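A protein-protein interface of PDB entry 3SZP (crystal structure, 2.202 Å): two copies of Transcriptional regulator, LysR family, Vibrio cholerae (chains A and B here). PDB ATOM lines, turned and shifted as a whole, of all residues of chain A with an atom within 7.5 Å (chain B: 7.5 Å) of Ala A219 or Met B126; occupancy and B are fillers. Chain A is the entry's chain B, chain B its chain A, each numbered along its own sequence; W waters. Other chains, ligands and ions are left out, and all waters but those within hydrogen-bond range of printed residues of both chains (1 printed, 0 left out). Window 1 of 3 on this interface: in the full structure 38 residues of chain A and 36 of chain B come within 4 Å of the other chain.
The backbone carbonyl oxygen of Ala A217 lies close to the side-chain sulfur of Met B26, 3.7 Å away. N of Leu B124 sits at hydrogen-bond distance from O of Gln A216 (2.7 Å). OG of Ser A218 sits at hydrogen-bond distance from N of Met B126. The side-chain sulfur (SD) of Met B26 is in hydrogen-bond range of the side-chain amide nitrogen (NE2) of Gln A216 (3.7 Å). The backbone NH (N) of Ser A218 sits at hydrogen-bond distance from the backbone carbonyl oxygen (O) of Leu B124 (2.9 Å). The side-chain sulfur of Met B26 is in hydrogen-bond range of the backbone NH of Ser A218 (3.7 Å).
The backbone NH (N) of Lys A190 lies within hydrogen-bond range of the backbone carbonyl oxygen (O) of Phe A215. The backbone NH (N) of Met B107 is in hydrogen-bond range of the backbone carbonyl oxygen (O) of Thr B102 (3.0 Å). The backbone NH (N) of Met B125 is in hydrogen-bond range of the backbone carbonyl oxygen (O) of Ile B95, at 2.9 Å. The side-chain amide nitrogen (ND2) of Asn A100 is in hydrogen-bond range of the backbone carbonyl oxygen (O) of Tyr A192, at 2.7 Å. O of Ala A217 is in hydrogen-bond range of N of Tyr A192 (2.8 Å). The side-chain amide nitrogen (ND2) of Asn A128 lies within hydrogen-bond range of the backbone carbonyl oxygen (O) of Ser A218, 3.1 Å away.
Among the printed residues, pairs that only touch across the chains: Ala A217 with Leu B124, Tyr A192 with Met B26, Asn A221 with Lys B103, Ser A218 with Met B125, Ala A219 with Met B126, Val A222 with Met B107, Val A222 with Met B126, Phe A215 with Met B107, Arg A224 with Lys B103, Phe A215 with Leu B124 and Val A222 with Lys B103.
Of chain B, only Met B126 comes within 4 Å of Ala A219. Met B126 touches just these residues of chain A: Ser A218, Ala A219 and Val A222. Of the printed residues of chain B, Ser A218 touches Met B26, Leu B124, Met B125 and Met B126. Of the printed residues of chain B, Arg A224 touches Lys B103 (3.8 Å). Printed residues of chain B within 4 Å of Gln A216: Met B26 (3.7 Å) and Leu B124 (2.7 Å). Of the printed residues of chain B, Phe A215 touches Met B107 and Leu B124. Printed residues of chain A within 4 Å of Lys B103: Asn A221 (3.4 Å), Val A222 (3.98 Å) and Arg A224 (3.8 Å). Pro A193 touches none of the printed residues of chain B. The nearest residue of chain B that does not touch Ala A219 is Leu B124 (5.2 Å). The nearest residue of chain A that does not touch Met B126 is Asn A221 (4.3 Å). The nearest printed residue of chain A that does not touch Met B26 is Pro A193 (5.5 Å).
Of the 19 printed residues of chain A, 9 touch a printed residue of chain B. Printed residues of chain B that touch a printed residue of chain A: Met B26, Lys B103, Met B107, Leu B124, Met B125 and Met B126. Hydrophobic or aromatic side chains of chain B within 4 Å of the printed part of chain A: Met B26, Met B107, Leu B124, Met B125 and Met B126. Along chain B the printed residues that touch a printed residue of chain A span positions 26 to 126. Among the printed residues, 17 pairs touch across the chains. Among the printed residues, no Asp or Glu carboxylate lies within 4 Å of a Lys or Arg side-chain nitrogen of the other chain.
Positions printed for both chains: 99, 100 and 128.
Water W1 lies within hydrogen-bond range of the side-chain hydroxyl (OG) of Ser A218 (2.9 Å) and the backbone carbonyl oxygen (O) of Met B126 (3.2 Å).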
ATOM      1  N   SER A  99      21.967  10.104 -14.056  1.00  0.00           N
ATOM      2  CA  SER A  99      22.742   8.904 -13.726  1.00  0.00           C
ATOM      3  C   SER A  99      24.238   9.108 -13.666  1.00  0.00           C
ATOM      4  O   SER A  99      24.867   8.754 -12.682  1.00  0.00           O
ATOM      5  CB  SER A  99      22.439   7.747 -14.681  1.00  0.00           C
ATOM      6  OG  SER A  99      21.074   7.403 -14.581  1.00  0.00           O
ATOM      7  N   ASN A 100      24.813   9.661 -14.724  1.00  0.00           N
ATOM      8  CA  ASN A 100      26.255   9.847 -14.762  1.00  0.00           C
ATOM      9  C   ASN A 100      26.806  10.697 -13.622  1.00  0.00           C
ATOM     10  O   ASN A 100      27.824  10.350 -13.026  1.00  0.00           O
ATOM     11  CB  ASN A 100      26.727  10.446 -16.091  1.00  0.00           C
ATOM     12  CG  ASN A 100      26.701   9.455 -17.237  1.00  0.00           C
ATOM     13  OD1 ASN A 100      26.984   8.261 -17.079  1.00  0.00           O
ATOM     14  ND2 ASN A 100      26.362   9.958 -18.417  1.00  0.00           N
ATOM     15  N   ASN A 128      19.149   8.505 -17.100  1.00  0.00           N
ATOM     16  CA  ASN A 128      19.868   9.112 -18.194  1.00  0.00           C
ATOM     17  C   ASN A 128      19.064  10.261 -18.787  1.00  0.00           C
ATOM     18  O   ASN A 128      19.647  11.194 -19.341  1.00  0.00           O
ATOM     19  CB  ASN A 128      20.191   8.060 -19.257  1.00  0.00           C
ATOM     20  CG  ASN A 128      21.597   7.498 -19.114  1.00  0.00           C
ATOM     21  OD1 ASN A 128      22.341   7.888 -18.208  1.00  0.00           O
ATOM     22  ND2 ASN A 128      21.974   6.584 -20.017  1.00  0.00           N
ATOM     23  N   LYS A 190      33.666   6.583 -25.946  1.00  0.00           N
ATOM     24  CA  LYS A 190      32.537   7.507 -25.943  1.00  0.00           C
ATOM     25  C   LYS A 190      31.416   6.988 -25.064  1.00  0.00           C
ATOM     26  O   LYS A 190      31.016   5.830 -25.183  1.00  0.00           O
ATOM     27  CB  LYS A 190      32.008   7.723 -27.361  1.00  0.00           C
ATOM     28  CG  LYS A 190      32.923   8.577 -28.251  1.00  0.00           C
ATOM     29  CD  LYS A 190      32.319   8.867 -29.628  1.00  0.00           C
ATOM     30  CE  LYS A 190      33.141   9.905 -30.386  1.00  0.00           C
ATOM     31  NZ  LYS A 190      32.549  10.313 -31.712  1.00  0.00           N
ATOM     32  N   GLY A 191      30.918   7.843 -24.181  1.00  0.00           N
ATOM     33  CA  GLY A 191      29.864   7.446 -23.280  1.00  0.00           C
ATOM     34  C   GLY A 191      28.672   8.400 -23.347  1.00  0.00           C
ATOM     35  O   GLY A 191      28.838   9.611 -23.476  1.00  0.00           O
ATOM     36  N   TYR A 192      27.473   7.841 -23.266  1.00  0.00           N
ATOM     37  CA  TYR A 192      26.264   8.648 -23.311  1.00  0.00           C
ATOM     38  C   TYR A 192      26.312   9.655 -22.164  1.00  0.00           C
ATOM     39  O   TYR A 192      26.687   9.287 -21.056  1.00  0.00           O
ATOM     40  CB  TYR A 192      25.060   7.734 -23.177  1.00  0.00           C
ATOM     41  CG  TYR A 192      23.758   8.469 -23.148  1.00  0.00           C
ATOM     42  CD1 TYR A 192      23.204   8.886 -21.950  1.00  0.00           C
ATOM     43  CD2 TYR A 192      23.076   8.748 -24.325  1.00  0.00           C
ATOM     44  CE1 TYR A 192      21.987   9.568 -21.924  1.00  0.00           C
ATOM     45  CE2 TYR A 192      21.889   9.427 -24.308  1.00  0.00           C
ATOM     46  CZ  TYR A 192      21.348   9.830 -23.110  1.00  0.00           C
ATOM     47  OH  TYR A 192      20.170  10.505 -23.117  1.00  0.00           O
ATOM     48  N   PRO A 193      25.917  10.919 -22.404  1.00  0.00           N
ATOM     49  CA  PRO A 193      25.335  11.537 -23.604  1.00  0.00           C
ATOM     50  C   PRO A 193      26.352  12.270 -24.466  1.00  0.00           C
ATOM     51  O   PRO A 193      25.981  13.153 -25.229  1.00  0.00           O
ATOM     52  CB  PRO A 193      24.360  12.555 -23.013  1.00  0.00           C
ATOM     53  CG  PRO A 193      25.080  13.057 -21.773  1.00  0.00           C
ATOM     54  CD  PRO A 193      25.855  11.824 -21.242  1.00  0.00           C
ATOM     55  N   PHE A 215      35.053   2.063 -28.167  1.00  0.00           N
ATOM     56  CA  PHE A 215      34.204   1.675 -27.052  1.00  0.00           C
ATOM     57  C   PHE A 215      33.118   2.736 -26.952  1.00  0.00           C
ATOM     58  O   PHE A 215      33.428   3.924 -26.928  1.00  0.00           O
ATOM     59  CB  PHE A 215      35.038   1.611 -25.766  1.00  0.00           C
ATOM     60  CG  PHE A 215      34.275   1.165 -24.550  1.00  0.00           C
ATOM     61  CD1 PHE A 215      33.401   0.093 -24.608  1.00  0.00           C
ATOM     62  CD2 PHE A 215      34.446   1.808 -23.334  1.00  0.00           C
ATOM     63  CE1 PHE A 215      32.689  -0.324 -23.472  1.00  0.00           C
ATOM     64  CE2 PHE A 215      33.741   1.385 -22.185  1.00  0.00           C
ATOM     65  CZ  PHE A 215      32.869   0.320 -22.263  1.00  0.00           C
ATOM     66  N   GLN A 216      31.859   2.309 -26.948  1.00  0.00           N
ATOM     67  CA  GLN A 216      30.720   3.204 -26.798  1.00  0.00           C
ATOM     68  C   GLN A 216      29.801   2.614 -25.738  1.00  0.00           C
ATOM     69  O   GLN A 216      29.387   1.464 -25.855  1.00  0.00           O
ATOM     70  CB  GLN A 216      29.960   3.341 -28.119  1.00  0.00           C
ATOM     71  CG  GLN A 216      28.653   4.153 -28.004  1.00  0.00           C
ATOM     72  CD  GLN A 216      27.828   4.199 -29.309  1.00  0.00           C
ATOM     73  OE1 GLN A 216      28.352   4.495 -30.390  1.00  0.00           O
ATOM     74  NE2 GLN A 216      26.523   3.919 -29.196  1.00  0.00           N
ATOM     75  N   ALA A 217      29.495   3.386 -24.698  1.00  0.00           N
ATOM     76  CA  ALA A 217      28.692   2.886 -23.587  1.00  0.00           C
ATOM     77  C   ALA A 217      27.551   3.830 -23.188  1.00  0.00           C
ATOM     78  O   ALA A 217      27.613   5.041 -23.444  1.00  0.00           O
ATOM     79  CB  ALA A 217      29.580   2.599 -22.374  1.00  0.00           C
ATOM     80  N   SER A 218      26.538   3.267 -22.528  1.00  0.00           N
ATOM     81  CA  SER A 218      25.396   4.055 -22.070  1.00  0.00           C
ATOM     82  C   SER A 218      25.715   4.840 -20.801  1.00  0.00           C
ATOM     83  O   SER A 218      24.887   5.594 -20.344  1.00  0.00           O
ATOM     84  CB  SER A 218      24.169   3.160 -21.822  1.00  0.00           C
ATOM     85  OG  SER A 218      24.445   2.200 -20.812  1.00  0.00           O
ATOM     86  N   ALA A 219      26.910   4.650 -20.234  1.00  0.00           N
ATOM     87  CA  ALA A 219      27.319   5.386 -19.032  1.00  0.00           C
ATOM     88  C   ALA A 219      28.801   5.792 -19.088  1.00  0.00           C
ATOM     89  O   ALA A 219      29.637   5.073 -19.652  1.00  0.00           O
ATOM     90  CB  ALA A 219      27.047   4.548 -17.788  1.00  0.00           C
ATOM     91  N   LEU A 220      29.133   6.942 -18.507  1.00  0.00           N
ATOM     92  CA  LEU A 220      30.485   7.471 -18.665  1.00  0.00           C
ATOM     93  C   LEU A 220      31.526   6.872 -17.716  1.00  0.00           C
ATOM     94  O   LEU A 220      32.714   6.860 -18.046  1.00  0.00           O
ATOM     95  CB  LEU A 220      30.500   9.006 -18.617  1.00  0.00           C
ATOM     96  CG  LEU A 220      30.103   9.732 -19.921  1.00  0.00           C
ATOM     97  CD1 LEU A 220      29.627  11.134 -19.628  1.00  0.00           C
ATOM     98  CD2 LEU A 220      31.257   9.741 -20.965  1.00  0.00           C
ATOM     99  N   ASN A 221      31.090   6.350 -16.567  1.00  0.00           N
ATOM    100  CA  ASN A 221      32.039   5.811 -15.603  1.00  0.00           C
ATOM    101  C   ASN A 221      32.837   4.618 -16.164  1.00  0.00           C
ATOM    102  O   ASN A 221      34.044   4.543 -15.965  1.00  0.00           O
ATOM    103  CB  ASN A 221      31.411   5.518 -14.234  1.00  0.00           C
ATOM    104  CG  ASN A 221      30.446   4.343 -14.253  1.00  0.00           C
ATOM    105  OD1 ASN A 221      30.010   3.892 -15.313  1.00  0.00           O
ATOM    106  ND2 ASN A 221      30.095   3.854 -13.065  1.00  0.00           N
ATOM    107  N   VAL A 222      32.174   3.736 -16.915  1.00  0.00           N
ATOM    108  CA  VAL A 222      32.867   2.609 -17.536  1.00  0.00           C
ATOM    109  C   VAL A 222      33.781   3.084 -18.682  1.00  0.00           C
ATOM    110  O   VAL A 222      34.772   2.450 -19.003  1.00  0.00           O
ATOM    111  CB  VAL A 222      31.885   1.525 -18.037  1.00  0.00           C
ATOM    112  CG1 VAL A 222      31.124   0.897 -16.866  1.00  0.00           C
ATOM    113  CG2 VAL A 222      30.913   2.113 -19.078  1.00  0.00           C
ATOM    114  N   VAL A 223      33.445   4.208 -19.293  1.00  0.00           N
ATOM    115  CA  VAL A 223      34.287   4.746 -20.361  1.00  0.00           C
ATOM    116  C   VAL A 223      35.585   5.304 -19.775  1.00  0.00           C
ATOM    117  O   VAL A 223      36.666   5.163 -20.357  1.00  0.00           O
ATOM    118  CB  VAL A 223      33.561   5.839 -21.162  1.00  0.00           C
ATOM    119  CG1 VAL A 223      34.524   6.529 -22.126  1.00  0.00           C
ATOM    120  CG2 VAL A 223      32.365   5.248 -21.915  1.00  0.00           C
ATOM    121  N   ARG A 224      35.455   5.935 -18.619  1.00  0.00           N
ATOM    122  CA  ARG A 224      36.573   6.523 -17.917  1.00  0.00           C
ATOM    123  C   ARG A 224      37.549   5.410 -17.529  1.00  0.00           C
ATOM    124  O   ARG A 224      38.758   5.554 -17.650  1.00  0.00           O
ATOM    125  CB  ARG A 224      36.084   7.249 -16.661  1.00  0.00           C
ATOM    126  CG  ARG A 224      37.193   7.988 -15.922  1.00  0.00           C
ATOM    127  CD  ARG A 224      36.681   8.593 -14.623  1.00  0.00           C
ATOM    128  NE  ARG A 224      36.197   7.564 -13.709  1.00  0.00           N
ATOM    129  CZ  ARG A 224      35.081   7.666 -12.993  1.00  0.00           C
ATOM    130  NH1 ARG A 224      34.337   8.771 -13.064  1.00  0.00           N
ATOM    131  NH2 ARG A 224      34.714   6.673 -12.202  1.00  0.00           N
ATOM    132  N   MET A 236      34.783  13.932 -21.339  1.00  0.00           N
ATOM    133  CA  MET A 236      34.195  13.596 -20.061  1.00  0.00           C
ATOM    134  C   MET A 236      34.069  14.823 -19.151  1.00  0.00           C
ATOM    135  O   MET A 236      34.950  15.673 -19.148  1.00  0.00           O
ATOM    136  CB  MET A 236      35.077  12.520 -19.434  1.00  0.00           C
ATOM    137  CG  MET A 236      34.756  12.145 -18.030  1.00  0.00           C
ATOM    138  SD  MET A 236      33.963  10.533 -17.973  1.00  0.00           S
ATOM    139  CE  MET A 236      35.018   9.543 -19.028  1.00  0.00           C
ATOM    140  N   MET A 240      33.683  14.479 -13.212  1.00  0.00           N
ATOM    141  CA  MET A 240      33.871  13.027 -13.116  1.00  0.00           C
ATOM    142  C   MET A 240      35.355  12.630 -13.122  1.00  0.00           C
ATOM    143  O   MET A 240      35.683  11.465 -12.968  1.00  0.00           O
ATOM    144  CB  MET A 240      33.129  12.303 -14.272  1.00  0.00           C
ATOM    145  CG  MET A 240      31.586  12.446 -14.242  1.00  0.00           C
ATOM    146  SD  MET A 240      30.644  11.462 -15.460  1.00  0.00           S
ATOM    147  CE  MET A 240      31.196   9.804 -15.017  1.00  0.00           C
ATOM    148  N   MET B  26      20.870   5.665 -27.722  1.00  0.00           N
ATOM    149  CA  MET B  26      21.875   6.509 -27.073  1.00  0.00           C
ATOM    150  C   MET B  26      21.978   7.905 -27.706  1.00  0.00           C
ATOM    151  O   MET B  26      23.036   8.546 -27.668  1.00  0.00           O
ATOM    152  CB  MET B  26      23.250   5.827 -27.022  1.00  0.00           C
ATOM    153  CG  MET B  26      23.280   4.472 -26.317  1.00  0.00           C
ATOM    154  SD  MET B  26      24.972   3.956 -25.837  1.00  0.00           S
ATOM    155  CE  MET B  26      24.725   2.171 -25.648  1.00  0.00           C
ATOM    156  N   ILE B  95      26.686  -5.497 -26.459  1.00  0.00           N
ATOM    157  CA  ILE B  95      26.581  -6.186 -25.188  1.00  0.00           C
ATOM    158  C   ILE B  95      25.629  -5.454 -24.245  1.00  0.00           C
ATOM    159  O   ILE B  95      25.672  -4.220 -24.154  1.00  0.00           O
ATOM    160  CB  ILE B  95      27.959  -6.252 -24.523  1.00  0.00           C
ATOM    161  CG1 ILE B  95      28.949  -6.945 -25.451  1.00  0.00           C
ATOM    162  CG2 ILE B  95      27.877  -6.960 -23.175  1.00  0.00           C
ATOM    163  CD1 ILE B  95      30.365  -6.905 -24.953  1.00  0.00           C
ATOM    164  N   SER B  96      24.776  -6.212 -23.556  1.00  0.00           N
ATOM    165  CA  SER B  96      23.950  -5.674 -22.483  1.00  0.00           C
ATOM    166  C   SER B  96      24.499  -6.194 -21.155  1.00  0.00           C
ATOM    167  O   SER B  96      24.943  -7.341 -21.073  1.00  0.00           O
ATOM    168  CB  SER B  96      22.486  -6.096 -22.663  1.00  0.00           C
ATOM    169  OG  SER B  96      21.716  -5.862 -21.497  1.00  0.00           O
ATOM    170  N   ALA B  97      24.491  -5.350 -20.122  1.00  0.00           N
ATOM    171  CA  ALA B  97      25.041  -5.733 -18.826  1.00  0.00           C
ATOM    172  C   ALA B  97      24.365  -4.970 -17.709  1.00  0.00           C
ATOM    173  O   ALA B  97      23.747  -3.932 -17.941  1.00  0.00           O
ATOM    174  CB  ALA B  97      26.563  -5.519 -18.784  1.00  0.00           C
ATOM    175  N   PRO B  98      24.475  -5.485 -16.477  1.00  0.00           N
ATOM    176  CA  PRO B  98      23.738  -4.853 -15.380  1.00  0.00           C
ATOM    177  C   PRO B  98      24.373  -3.535 -14.973  1.00  0.00           C
ATOM    178  O   PRO B  98      25.584  -3.351 -15.123  1.00  0.00           O
ATOM    179  CB  PRO B  98      23.839  -5.883 -14.252  1.00  0.00           C
ATOM    180  CG  PRO B  98      25.031  -6.661 -14.539  1.00  0.00           C
ATOM    181  CD  PRO B  98      25.178  -6.706 -16.044  1.00  0.00           C
ATOM    182  N   SER B  99      23.559  -2.622 -14.472  1.00  0.00           N
ATOM    183  CA  SER B  99      24.050  -1.330 -14.017  1.00  0.00           C
ATOM    184  C   SER B  99      25.023  -1.442 -12.864  1.00  0.00           C
ATOM    185  O   SER B  99      26.071  -0.828 -12.892  1.00  0.00           O
ATOM    186  CB  SER B  99      22.892  -0.423 -13.586  1.00  0.00           C
ATOM    187  OG  SER B  99      22.163   0.006 -14.707  1.00  0.00           O
ATOM    188  N   ASN B 100      24.684  -2.206 -11.838  1.00  0.00           N
ATOM    189  CA  ASN B 100      25.522  -2.193 -10.644  1.00  0.00           C
ATOM    190  C   ASN B 100      26.933  -2.754 -10.808  1.00  0.00           C
ATOM    191  O   ASN B 100      27.902  -2.101 -10.406  1.00  0.00           O
ATOM    192  CB  ASN B 100      24.821  -2.852  -9.458  1.00  0.00           C
ATOM    193  CG  ASN B 100      23.625  -2.057  -8.995  1.00  0.00           C
ATOM    194  OD1 ASN B 100      23.628  -0.826  -9.057  1.00  0.00           O
ATOM    195  ND2 ASN B 100      22.580  -2.753  -8.566  1.00  0.00           N
ATOM    196  N   LEU B 101      27.070  -3.939 -11.391  1.00  0.00           N
ATOM    197  CA  LEU B 101      28.308  -4.684 -11.169  1.00  0.00           C
ATOM    198  C   LEU B 101      29.330  -4.523 -12.276  1.00  0.00           C
ATOM    199  O   LEU B 101      30.483  -4.945 -12.160  1.00  0.00           O
ATOM    200  CB  LEU B 101      27.995  -6.168 -10.967  1.00  0.00           C
ATOM    201  CG  LEU B 101      27.097  -6.465  -9.768  1.00  0.00           C
ATOM    202  CD1 LEU B 101      26.617  -7.907  -9.803  1.00  0.00           C
ATOM    203  CD2 LEU B 101      27.853  -6.179  -8.488  1.00  0.00           C
ATOM    204  N   THR B 102      28.900  -3.914 -13.360  1.00  0.00           N
ATOM    205  CA  THR B 102      29.695  -3.946 -14.566  1.00  0.00           C
ATOM    206  C   THR B 102      31.031  -3.248 -14.391  1.00  0.00           C
ATOM    207  O   THR B 102      32.061  -3.776 -14.785  1.00  0.00           O
ATOM    208  CB  THR B 102      28.904  -3.372 -15.744  1.00  0.00           C
ATOM    209  OG1 THR B 102      27.829  -4.263 -16.010  1.00  0.00           O
ATOM    210  CG2 THR B 102      29.755  -3.284 -16.982  1.00  0.00           C
ATOM    211  N   LYS B 103      30.995  -2.061 -13.810  1.00  0.00           N
ATOM    212  CA  LYS B 103      32.178  -1.236 -13.672  1.00  0.00           C
ATOM    213  C   LYS B 103      33.295  -2.026 -12.986  1.00  0.00           C
ATOM    214  O   LYS B 103      34.391  -2.172 -13.524  1.00  0.00           O
ATOM    215  CB  LYS B 103      31.822   0.028 -12.891  1.00  0.00           C
ATOM    216  CG  LYS B 103      33.004   0.886 -12.451  1.00  0.00           C
ATOM    217  CD  LYS B 103      33.462   1.834 -13.535  1.00  0.00           C
ATOM    218  CE  LYS B 103      34.283   2.964 -12.930  1.00  0.00           C
ATOM    219  NZ  LYS B 103      35.315   2.410 -11.988  1.00  0.00           N
ATOM    220  N   MET B 107      34.410  -4.684 -16.383  1.00  0.00           N
ATOM    221  CA  MET B 107      35.272  -3.796 -17.173  1.00  0.00           C
ATOM    222  C   MET B 107      36.730  -4.259 -17.271  1.00  0.00           C
ATOM    223  O   MET B 107      37.332  -4.142 -18.333  1.00  0.00           O
ATOM    224  CB  MET B 107      35.211  -2.353 -16.668  1.00  0.00           C
ATOM    225  CG  MET B 107      33.968  -1.596 -17.094  1.00  0.00           C
ATOM    226  SD  MET B 107      33.612  -1.688 -18.856  1.00  0.00           S
ATOM    227  CE  MET B 107      35.144  -1.082 -19.590  1.00  0.00           C
ATOM    228  N   PHE B 110      36.454  -6.624 -20.006  1.00  0.00           N
ATOM    229  CA  PHE B 110      36.123  -5.972 -21.259  1.00  0.00           C
ATOM    230  C   PHE B 110      37.334  -5.194 -21.766  1.00  0.00           C
ATOM    231  O   PHE B 110      37.624  -5.179 -22.958  1.00  0.00           O
ATOM    232  CB  PHE B 110      34.918  -5.023 -21.096  1.00  0.00           C
ATOM    233  CG  PHE B 110      33.622  -5.734 -20.809  1.00  0.00           C
ATOM    234  CD1 PHE B 110      33.546  -7.114 -20.897  1.00  0.00           C
ATOM    235  CD2 PHE B 110      32.462  -5.023 -20.482  1.00  0.00           C
ATOM    236  CE1 PHE B 110      32.343  -7.787 -20.651  1.00  0.00           C
ATOM    237  CE2 PHE B 110      31.254  -5.695 -20.235  1.00  0.00           C
ATOM    238  CZ  PHE B 110      31.199  -7.073 -20.309  1.00  0.00           C
ATOM    239  N   LEU B 124      28.356  -1.010 -25.361  1.00  0.00           N
ATOM    240  CA  LEU B 124      27.907  -1.557 -24.084  1.00  0.00           C
ATOM    241  C   LEU B 124      26.725  -0.757 -23.513  1.00  0.00           C
ATOM    242  O   LEU B 124      26.828   0.447 -23.287  1.00  0.00           O
ATOM    243  CB  LEU B 124      29.068  -1.558 -23.089  1.00  0.00           C
ATOM    244  CG  LEU B 124      28.806  -2.010 -21.645  1.00  0.00           C
ATOM    245  CD1 LEU B 124      28.393  -3.481 -21.598  1.00  0.00           C
ATOM    246  CD2 LEU B 124      30.037  -1.783 -20.787  1.00  0.00           C
ATOM    247  N   MET B 125      25.604  -1.439 -23.309  1.00  0.00           N
ATOM    248  CA  MET B 125      24.424  -0.841 -22.701  1.00  0.00           C
ATOM    249  C   MET B 125      24.172  -1.430 -21.314  1.00  0.00           C
ATOM    250  O   MET B 125      24.031  -2.637 -21.156  1.00  0.00           O
ATOM    251  CB  MET B 125      23.200  -1.064 -23.585  1.00  0.00           C
ATOM    252  CG  MET B 125      21.886  -0.727 -22.908  1.00  0.00           C
ATOM    253  SD  MET B 125      21.515   1.044 -22.946  1.00  0.00           S
ATOM    254  CE  MET B 125      21.353   1.322 -24.722  1.00  0.00           C
ATOM    255  N   MET B 126      24.124  -0.564 -20.310  1.00  0.00           N
ATOM    256  CA  MET B 126      23.834  -0.989 -18.948  1.00  0.00           C
ATOM    257  C   MET B 126      22.397  -0.715 -18.559  1.00  0.00           C
ATOM    258  O   MET B 126      21.864   0.354 -18.851  1.00  0.00           O
ATOM    259  CB  MET B 126      24.748  -0.280 -17.959  1.00  0.00           C
ATOM    260  CG  MET B 126      25.912  -1.126 -17.555  1.00  0.00           C
ATOM    261  SD  MET B 126      27.396  -0.428 -18.250  1.00  0.00           S
ATOM    262  CE  MET B 126      27.487   1.037 -17.207  1.00  0.00           C
ATOM    263  N   SER B 127      21.780  -1.665 -17.869  1.00  0.00           N
ATOM    264  CA  SER B 127      20.448  -1.439 -17.300  1.00  0.00           C
ATOM    265  C   SER B 127      20.213  -2.318 -16.076  1.00  0.00           C
ATOM    266  O   SER B 127      20.827  -3.367 -15.933  1.00  0.00           O
ATOM    267  CB  SER B 127      19.374  -1.726 -18.349  1.00  0.00           C
ATOM    268  OG  SER B 127      19.658  -2.972 -18.965  1.00  0.00           O
ATOM    269  N   ASN B 128      19.313  -1.888 -15.196  1.00  0.00           N
ATOM    270  CA  ASN B 128      18.900  -2.738 -14.091  1.00  0.00           C
ATOM    271  C   ASN B 128      18.275  -3.995 -14.696  1.00  0.00           C
ATOM    272  O   ASN B 128      17.884  -3.993 -15.869  1.00  0.00           O
ATOM    273  CB  ASN B 128      17.923  -1.998 -13.186  1.00  0.00           C
ATOM    274  CG  ASN B 128      16.605  -1.694 -13.876  1.00  0.00           C
ATOM    275  OD1 ASN B 128      16.502  -1.773 -15.101  1.00  0.00           O
ATOM    276  ND2 ASN B 128      15.586  -1.347 -13.094  1.00  0.00           N
ATOM    277  N   TRP B 138      21.048  -8.244 -29.472  1.00  0.00           N
ATOM    278  CA  TRP B 138      22.306  -8.203 -28.739  1.00  0.00           C
ATOM    279  C   TRP B 138      23.199  -9.353 -29.161  1.00  0.00           C
ATOM    280  O   TRP B 138      22.702 -10.416 -29.538  1.00  0.00           O
ATOM    281  CB  TRP B 138      22.025  -8.299 -27.240  1.00  0.00           C
ATOM    282  CG  TRP B 138      21.088  -7.237 -26.768  1.00  0.00           C
ATOM    283  CD1 TRP B 138      19.728  -7.330 -26.640  1.00  0.00           C
ATOM    284  CD2 TRP B 138      21.438  -5.908 -26.393  1.00  0.00           C
ATOM    285  NE1 TRP B 138      19.211  -6.133 -26.194  1.00  0.00           N
ATOM    286  CE2 TRP B 138      20.247  -5.244 -26.029  1.00  0.00           C
ATOM    287  CE3 TRP B 138      22.651  -5.210 -26.321  1.00  0.00           C
ATOM    288  CZ2 TRP B 138      20.226  -3.912 -25.615  1.00  0.00           C
ATOM    289  CZ3 TRP B 138      22.632  -3.897 -25.900  1.00  0.00           C
ATOM    290  CH2 TRP B 138      21.425  -3.256 -25.560  1.00  0.00           C
HETATM  291  O   HOH W   1      23.214   3.209 -18.380  1.00  0.00           O
